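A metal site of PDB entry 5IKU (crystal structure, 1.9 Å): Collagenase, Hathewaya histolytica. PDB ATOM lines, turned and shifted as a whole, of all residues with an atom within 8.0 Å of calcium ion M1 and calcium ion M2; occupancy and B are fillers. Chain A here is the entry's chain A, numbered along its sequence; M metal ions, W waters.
Within 4 Å of calcium ion M1: Glu 133, Asn 135, Asp 136, Asp 159, Arg 161 and Asp 162.
Calcium ion M1 is bound by the side-chain amide oxygen (OD1) of Asn 135 (2.4 Å), the backbone carbonyl oxygen (O) of Arg 161 (2.4 Å), the side-chain carboxylate (OE2) of Glu 133 (2.4 Å), the side-chain carboxylate (OD1) of Asp 162 (2.4 Å), the side-chain carboxylate (OD1) of Asp 159 (2.4 Å), the side-chain carboxylate (OD2) of Asp 136 (2.4 Å) and the side-chain carboxylate (OE1) of Glu 133 (2.7 Å). Calcium ion M1 has seven donor atoms within binding distance.
Within 4 Å of calcium ion M2: Glu 131, Glu 133, Ser 154, Asp 159 and Asp 162. The nearest printed residue that does not touch calcium ion M2 is Leu 155 (4.4 Å).
ND2 of Asn 135 sits close to OE1 of Glu 131 (3.0 Å). The backbone carbonyl oxygen (O) of Asn 135 sits at hydrogen-bond distance from the backbone NH (N) of Tyr 163 (3.0 Å). The side-chain amide nitrogen (ND2) of Asn 135 lies within hydrogen-bond range of the side-chain hydroxyl (OG1) of Thr 142 (3.1 Å). OD2 of Asp 162 sits close to OH of Tyr 234 (2.5 Å). O of Asp 162 is in hydrogen-bond range of N of Val 225. The backbone NH (N) of Asp 136 is in hydrogen-bond range of the side-chain amide oxygen (OD1) of Asn 134, 3.0 Å away. The backbone NH (N) of Glu 131 lies within hydrogen-bond range of the backbone carbonyl oxygen (O) of Gln 152 (3.1 Å).
The backbone carbonyl oxygen (O) of Ser 154 binds calcium ion M2 (2.2 Å). Calcium ion M2 is bound by OD2 of Asp 159. The side-chain carboxylate (OE2) of Glu 133 binds calcium ion M2, at 2.4 Å. OD1 of Asp 162 is bound to calcium ion M2 (2.5 Å). The side-chain carboxylate (OE2) of Glu 131 binds calcium ion M2. Calcium ion M2 is bound by water W1, 2.5 Å away. The side-chain carboxylate (OE1) of Glu 131 is bound to calcium ion M2 (2.6 Å). OD2 of Asp 162 is bound to calcium ion M2 (2.7 Å). Calcium ion M2 has eight donor atoms within binding distance.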
ATOM      1  N   GLU A 131      13.149  17.550   9.696  1.00  0.00           N
ATOM      2  CA  GLU A 131      11.751  17.277   9.332  1.00  0.00           C
ATOM      3  C   GLU A 131      11.510  17.806   7.921  1.00  0.00           C
ATOM      4  O   GLU A 131      12.279  18.635   7.399  1.00  0.00           O
ATOM      5  CB  GLU A 131      10.787  18.028  10.253  1.00  0.00           C
ATOM      6  CG  GLU A 131      10.999  19.527  10.232  1.00  0.00           C
ATOM      7  CD  GLU A 131       9.865  20.269  10.957  1.00  0.00           C
ATOM      8  OE1 GLU A 131       8.697  19.806  10.903  1.00  0.00           O
ATOM      9  OE2 GLU A 131      10.135  21.336  11.557  1.00  0.00           O
ATOM     10  N   LYS A 132      10.446  17.296   7.316  1.00  0.00           N
ATOM     11  CA  LYS A 132      10.075  17.667   5.947  1.00  0.00           C
ATOM     12  C   LYS A 132       8.681  18.283   5.916  1.00  0.00           C
ATOM     13  O   LYS A 132       7.670  17.585   5.967  1.00  0.00           O
ATOM     14  CB  LYS A 132      10.124  16.449   5.046  1.00  0.00           C
ATOM     15  CG  LYS A 132      11.515  15.838   5.040  1.00  0.00           C
ATOM     16  CD  LYS A 132      11.640  14.786   3.950  1.00  0.00           C
ATOM     17  CE  LYS A 132      13.006  14.108   4.073  1.00  0.00           C
ATOM     18  NZ  LYS A 132      14.073  15.019   3.562  1.00  0.00           N
ATOM     19  N   GLU A 133       8.626  19.582   5.809  1.00  0.00           N
ATOM     20  CA  GLU A 133       7.316  20.231   5.682  1.00  0.00           C
ATOM     21  C   GLU A 133       6.833  20.044   4.221  1.00  0.00           C
ATOM     22  O   GLU A 133       7.651  19.830   3.361  1.00  0.00           O
ATOM     23  CB  GLU A 133       7.484  21.694   6.065  1.00  0.00           C
ATOM     24  CG  GLU A 133       7.712  21.816   7.563  1.00  0.00           C
ATOM     25  CD  GLU A 133       6.450  21.653   8.429  1.00  0.00           C
ATOM     26  OE1 GLU A 133       5.324  21.413   7.929  1.00  0.00           O
ATOM     27  OE2 GLU A 133       6.583  21.770   9.665  1.00  0.00           O
ATOM     28  N   ASN A 134       5.530  20.073   3.935  1.00  0.00           N
ATOM     29  CA  ASN A 134       4.446  20.205   4.925  1.00  0.00           C
ATOM     30  C   ASN A 134       4.195  18.855   5.604  1.00  0.00           C
ATOM     31  O   ASN A 134       4.017  17.871   4.918  1.00  0.00           O
ATOM     32  CB  ASN A 134       3.188  20.582   4.115  1.00  0.00           C
ATOM     33  CG  ASN A 134       2.037  21.046   4.978  1.00  0.00           C
ATOM     34  OD1 ASN A 134       1.646  20.425   5.946  1.00  0.00           O
ATOM     35  ND2 ASN A 134       1.455  22.152   4.579  1.00  0.00           N
ATOM     36  N   ASN A 135       4.158  18.791   6.939  1.00  0.00           N
ATOM     37  CA  ASN A 135       3.864  17.512   7.595  1.00  0.00           C
ATOM     38  C   ASN A 135       2.714  17.686   8.587  1.00  0.00           C
ATOM     39  O   ASN A 135       2.668  17.011   9.617  1.00  0.00           O
ATOM     40  CB  ASN A 135       5.123  16.946   8.322  1.00  0.00           C
ATOM     41  CG  ASN A 135       5.805  17.969   9.212  1.00  0.00           C
ATOM     42  OD1 ASN A 135       5.221  18.998   9.572  1.00  0.00           O
ATOM     43  ND2 ASN A 135       7.070  17.686   9.582  1.00  0.00           N
ATOM     44  N   ASP A 136       1.782  18.583   8.251  1.00  0.00           N
ATOM     45  CA  ASP A 136       0.714  18.956   9.179  1.00  0.00           C
ATOM     46  C   ASP A 136      -0.436  17.950   9.314  1.00  0.00           C
ATOM     47  O   ASP A 136      -1.318  18.150  10.144  1.00  0.00           O
ATOM     48  CB  ASP A 136       0.112  20.319   8.793  1.00  0.00           C
ATOM     49  CG  ASP A 136       1.161  21.439   8.782  1.00  0.00           C
ATOM     50  OD1 ASP A 136       0.825  22.528   8.293  1.00  0.00           O
ATOM     51  OD2 ASP A 136       2.289  21.243   9.260  1.00  0.00           O
ATOM     52  N   SER A 137      -0.448  16.874   8.524  1.00  0.00           N
ATOM     53  CA  SER A 137      -1.451  15.837   8.700  1.00  0.00           C
ATOM     54  C   SER A 137      -0.765  14.470   8.601  1.00  0.00           C
ATOM     55  O   SER A 137       0.361  14.361   8.098  1.00  0.00           O
ATOM     56  CB  SER A 137      -2.571  15.994   7.663  1.00  0.00           C
ATOM     57  OG  SER A 137      -1.983  16.028   6.378  1.00  0.00           O
ATOM     58  N   LYS A 140       0.947  13.175   5.524  1.00  0.00           N
ATOM     59  CA  LYS A 140       2.169  13.865   5.101  1.00  0.00           C
ATOM     60  C   LYS A 140       3.288  13.728   6.177  1.00  0.00           C
ATOM     61  O   LYS A 140       4.204  14.543   6.234  1.00  0.00           O
ATOM     62  CB  LYS A 140       1.851  15.326   4.717  1.00  0.00           C
ATOM     63  CG  LYS A 140       1.085  15.489   3.391  1.00  0.00           C
ATOM     64  CD  LYS A 140       0.693  16.915   3.013  1.00  0.00           C
ATOM     65  CE  LYS A 140      -0.762  17.274   3.299  1.00  0.00           C
ATOM     66  NZ  LYS A 140      -0.976  17.675   4.717  1.00  0.00           N
ATOM     67  N   THR A 142       6.498  12.989   8.422  1.00  0.00           N
ATOM     68  CA  THR A 142       7.891  12.809   8.094  1.00  0.00           C
ATOM     69  C   THR A 142       8.324  11.458   8.675  1.00  0.00           C
ATOM     70  O   THR A 142       8.140  11.205   9.857  1.00  0.00           O
ATOM     71  CB  THR A 142       8.715  13.914   8.780  1.00  0.00           C
ATOM     72  OG1 THR A 142       8.291  15.162   8.241  1.00  0.00           O
ATOM     73  CG2 THR A 142      10.256  13.645   8.606  1.00  0.00           C
ATOM     74  N   GLN A 152      15.526  17.007  13.646  1.00  0.00           N
ATOM     75  CA  GLN A 152      15.574  18.411  14.041  1.00  0.00           C
ATOM     76  C   GLN A 152      14.317  19.092  13.486  1.00  0.00           C
ATOM     77  O   GLN A 152      14.065  19.025  12.297  1.00  0.00           O
ATOM     78  CB  GLN A 152      16.821  19.066  13.429  1.00  0.00           C
ATOM     79  CG  GLN A 152      18.113  18.441  13.936  1.00  0.00           C
ATOM     80  CD  GLN A 152      19.369  18.956  13.251  1.00  0.00           C
ATOM     81  OE1 GLN A 152      19.506  18.970  12.005  1.00  0.00           O
ATOM     82  NE2 GLN A 152      20.328  19.369  14.065  1.00  0.00           N
ATOM     83  N   GLY A 153      13.527  19.743  14.348  1.00  0.00           N
ATOM     84  CA  GLY A 153      12.345  20.394  13.846  1.00  0.00           C
ATOM     85  C   GLY A 153      12.101  21.736  14.482  1.00  0.00           C
ATOM     86  O   GLY A 153      12.776  22.114  15.427  1.00  0.00           O
ATOM     87  N   SER A 154      11.126  22.471  13.947  1.00  0.00           N
ATOM     88  CA  SER A 154      10.686  23.716  14.588  1.00  0.00           C
ATOM     89  C   SER A 154       9.180  23.843  14.382  1.00  0.00           C
ATOM     90  O   SER A 154       8.597  23.243  13.448  1.00  0.00           O
ATOM     91  CB  SER A 154      11.363  24.959  13.991  1.00  0.00           C
ATOM     92  OG  SER A 154      11.034  25.029  12.623  1.00  0.00           O
ATOM     93  N   LEU A 155       8.596  24.643  15.263  1.00  0.00           N
ATOM     94  CA  LEU A 155       7.173  24.989  15.274  1.00  0.00           C
ATOM     95  C   LEU A 155       7.119  26.512  15.484  1.00  0.00           C
ATOM     96  O   LEU A 155       6.808  26.997  16.585  1.00  0.00           O
ATOM     97  CB  LEU A 155       6.484  24.280  16.446  1.00  0.00           C
ATOM     98  CG  LEU A 155       6.376  22.764  16.328  1.00  0.00           C
ATOM     99  CD1 LEU A 155       6.085  22.147  17.689  1.00  0.00           C
ATOM    100  CD2 LEU A 155       5.288  22.423  15.308  1.00  0.00           C
ATOM    101  N   LEU A 156       7.467  27.252  14.439  1.00  0.00           N
ATOM    102  CA  LEU A 156       7.509  28.718  14.520  1.00  0.00           C
ATOM    103  C   LEU A 156       6.235  29.272  13.879  1.00  0.00           C
ATOM    104  O   LEU A 156       5.778  28.746  12.870  1.00  0.00           O
ATOM    105  CB  LEU A 156       8.773  29.255  13.829  1.00  0.00           C
ATOM    106  CG  LEU A 156      10.088  28.578  14.262  1.00  0.00           C
ATOM    107  CD1 LEU A 156      11.186  28.927  13.282  1.00  0.00           C
ATOM    108  CD2 LEU A 156      10.473  28.978  15.672  1.00  0.00           C
ATOM    109  N   ASP A 158       2.921  30.059  12.265  1.00  0.00           N
ATOM    110  CA  ASP A 158       1.741  29.369  11.734  1.00  0.00           C
ATOM    111  C   ASP A 158       1.822  27.872  11.968  1.00  0.00           C
ATOM    112  O   ASP A 158       0.790  27.219  12.086  1.00  0.00           O
ATOM    113  CB  ASP A 158       1.640  29.570  10.224  1.00  0.00           C
ATOM    114  CG  ASP A 158       1.171  30.935   9.866  1.00  0.00           C
ATOM    115  OD1 ASP A 158       1.594  31.923  10.501  1.00  0.00           O
ATOM    116  OD2 ASP A 158       0.375  31.026   8.913  1.00  0.00           O
ATOM    117  N   ASP A 159       3.050  27.358  12.013  1.00  0.00           N
ATOM    118  CA  ASP A 159       3.322  25.932  12.096  1.00  0.00           C
ATOM    119  C   ASP A 159       3.154  25.443  13.525  1.00  0.00           C
ATOM    120  O   ASP A 159       3.983  25.759  14.391  1.00  0.00           O
ATOM    121  CB  ASP A 159       4.770  25.682  11.634  1.00  0.00           C
ATOM    122  CG  ASP A 159       5.111  24.214  11.493  1.00  0.00           C
ATOM    123  OD1 ASP A 159       4.282  23.404  11.022  1.00  0.00           O
ATOM    124  OD2 ASP A 159       6.259  23.872  11.845  1.00  0.00           O
ATOM    125  N   SER A 160       2.097  24.662  13.764  1.00  0.00           N
ATOM    126  CA  SER A 160       1.767  24.190  15.115  1.00  0.00           C
ATOM    127  C   SER A 160       1.697  22.675  15.269  1.00  0.00           C
ATOM    128  O   SER A 160       1.609  22.180  16.392  1.00  0.00           O
ATOM    129  CB  SER A 160       0.420  24.808  15.582  1.00  0.00           C
ATOM    130  OG  SER A 160      -0.631  24.221  14.815  1.00  0.00           O
ATOM    131  N   ARG A 161       1.755  21.931  14.159  1.00  0.00           N
ATOM    132  CA  ARG A 161       1.766  20.474  14.221  1.00  0.00           C
ATOM    133  C   ARG A 161       2.839  19.931  13.301  1.00  0.00           C
ATOM    134  O   ARG A 161       2.936  20.370  12.166  1.00  0.00           O
ATOM    135  CB  ARG A 161       0.469  19.900  13.692  1.00  0.00           C
ATOM    136  CG  ARG A 161      -0.750  20.467  14.405  1.00  0.00           C
ATOM    137  CD  ARG A 161      -1.919  20.623  13.443  1.00  0.00           C
ATOM    138  NE  ARG A 161      -2.771  19.452  13.460  1.00  0.00           N
ATOM    139  CZ  ARG A 161      -3.645  19.175  14.430  1.00  0.00           C
ATOM    140  NH1 ARG A 161      -3.783  19.969  15.477  1.00  0.00           N
ATOM    141  NH2 ARG A 161      -4.388  18.088  14.336  1.00  0.00           N
ATOM    142  N   ASP A 162       3.607  18.956  13.778  1.00  0.00           N
ATOM    143  CA  ASP A 162       4.546  18.219  12.924  1.00  0.00           C
ATOM    144  C   ASP A 162       4.232  16.768  13.195  1.00  0.00           C
ATOM    145  O   ASP A 162       4.387  16.290  14.330  1.00  0.00           O
ATOM    146  CB  ASP A 162       6.002  18.452  13.345  1.00  0.00           C
ATOM    147  CG  ASP A 162       6.480  19.873  13.089  1.00  0.00           C
ATOM    148  OD1 ASP A 162       5.921  20.560  12.228  1.00  0.00           O
ATOM    149  OD2 ASP A 162       7.442  20.333  13.738  1.00  0.00           O
ATOM    150  N   TYR A 163       3.791  16.043  12.168  1.00  0.00           N
ATOM    151  CA  TYR A 163       3.570  14.603  12.324  1.00  0.00           C
ATOM    152  C   TYR A 163       4.783  13.852  11.822  1.00  0.00           C
ATOM    153  O   TYR A 163       5.372  14.207  10.790  1.00  0.00           O
ATOM    154  CB  TYR A 163       2.447  14.143  11.410  1.00  0.00           C
ATOM    155  CG  TYR A 163       1.069  14.253  11.986  1.00  0.00           C
ATOM    156  CD1 TYR A 163       0.291  15.385  11.770  1.00  0.00           C
ATOM    157  CD2 TYR A 163       0.539  13.216  12.733  1.00  0.00           C
ATOM    158  CE1 TYR A 163      -0.985  15.484  12.294  1.00  0.00           C
ATOM    159  CE2 TYR A 163      -0.744  13.283  13.243  1.00  0.00           C
ATOM    160  CZ  TYR A 163      -1.488  14.422  13.034  1.00  0.00           C
ATOM    161  OH  TYR A 163      -2.757  14.474  13.553  1.00  0.00           O
ATOM    162  N   TYR A 164       5.131  12.801  12.543  1.00  0.00           N
ATOM    163  CA  TYR A 164       6.242  11.928  12.167  1.00  0.00           C
ATOM    164  C   TYR A 164       5.652  10.522  12.145  1.00  0.00           C
ATOM    165  O   TYR A 164       4.641  10.291  12.791  1.00  0.00           O
ATOM    166  CB  TYR A 164       7.347  12.000  13.251  1.00  0.00           C
ATOM    167  CG  TYR A 164       8.096  13.312  13.294  1.00  0.00           C
ATOM    168  CD1 TYR A 164       7.615  14.378  14.091  1.00  0.00           C
ATOM    169  CD2 TYR A 164       9.266  13.517  12.546  1.00  0.00           C
ATOM    170  CE1 TYR A 164       8.296  15.573  14.143  1.00  0.00           C
ATOM    171  CE2 TYR A 164       9.945  14.719  12.604  1.00  0.00           C
ATOM    172  CZ  TYR A 164       9.446  15.731  13.423  1.00  0.00           C
ATOM    173  OH  TYR A 164      10.089  16.936  13.494  1.00  0.00           O
ATOM    174  N   LEU A 224       2.532  12.811  16.792  1.00  0.00           N
ATOM    175  CA  LEU A 224       2.219  14.207  16.518  1.00  0.00           C
ATOM    176  C   LEU A 224       2.934  15.143  17.524  1.00  0.00           C
ATOM    177  O   LEU A 224       2.700  15.048  18.724  1.00  0.00           O
ATOM    178  CB  LEU A 224       0.690  14.422  16.583  1.00  0.00           C
ATOM    179  CG  LEU A 224       0.163  15.848  16.751  1.00  0.00           C
ATOM    180  CD1 LEU A 224       0.532  16.701  15.552  1.00  0.00           C
ATOM    181  CD2 LEU A 224      -1.333  15.872  16.941  1.00  0.00           C
ATOM    182  N   VAL A 225       3.801  16.037  17.051  1.00  0.00           N
ATOM    183  CA  VAL A 225       4.462  17.009  17.927  1.00  0.00           C
ATOM    184  C   VAL A 225       3.648  18.262  17.698  1.00  0.00           C
ATOM    185  O   VAL A 225       3.437  18.675  16.564  1.00  0.00           O
ATOM    186  CB  VAL A 225       5.941  17.241  17.529  1.00  0.00           C
ATOM    187  CG1 VAL A 225       6.588  18.283  18.429  1.00  0.00           C
ATOM    188  CG2 VAL A 225       6.712  15.925  17.603  1.00  0.00           C
ATOM    189  N   GLY A 232       9.177  27.677  18.909  1.00  0.00           N
ATOM    190  CA  GLY A 232      10.523  27.269  19.189  1.00  0.00           C
ATOM    191  C   GLY A 232      10.955  26.069  18.349  1.00  0.00           C
ATOM    192  O   GLY A 232      10.179  25.551  17.534  1.00  0.00           O
ATOM    193  N   TYR A 234      13.100  22.150  18.395  1.00  0.00           N
ATOM    194  CA  TYR A 234      13.215  20.973  19.251  1.00  0.00           C
ATOM    195  C   TYR A 234      14.033  19.925  18.494  1.00  0.00           C
ATOM    196  O   TYR A 234      14.257  20.046  17.275  1.00  0.00           O
ATOM    197  CB  TYR A 234      11.811  20.438  19.555  1.00  0.00           C
ATOM    198  CG  TYR A 234      11.033  20.002  18.325  1.00  0.00           C
ATOM    199  CD1 TYR A 234      10.184  20.892  17.653  1.00  0.00           C
ATOM    200  CD2 TYR A 234      11.167  18.716  17.813  1.00  0.00           C
ATOM    201  CE1 TYR A 234       9.492  20.492  16.533  1.00  0.00           C
ATOM    202  CE2 TYR A 234      10.477  18.326  16.683  1.00  0.00           C
ATOM    203  CZ  TYR A 234       9.646  19.223  16.043  1.00  0.00           C
ATOM    204  OH  TYR A 234       8.973  18.803  14.938  1.00  0.00           O
HETATM  205 CA    CA M   1       4.409  21.069  10.412  1.00  0.00          CA
HETATM  206 CA    CA M   2       7.786  22.065  11.718  1.00  0.00          CA
HETATM  207  O   HOH W   1       8.916  23.662  10.172  1.00  0.00           O
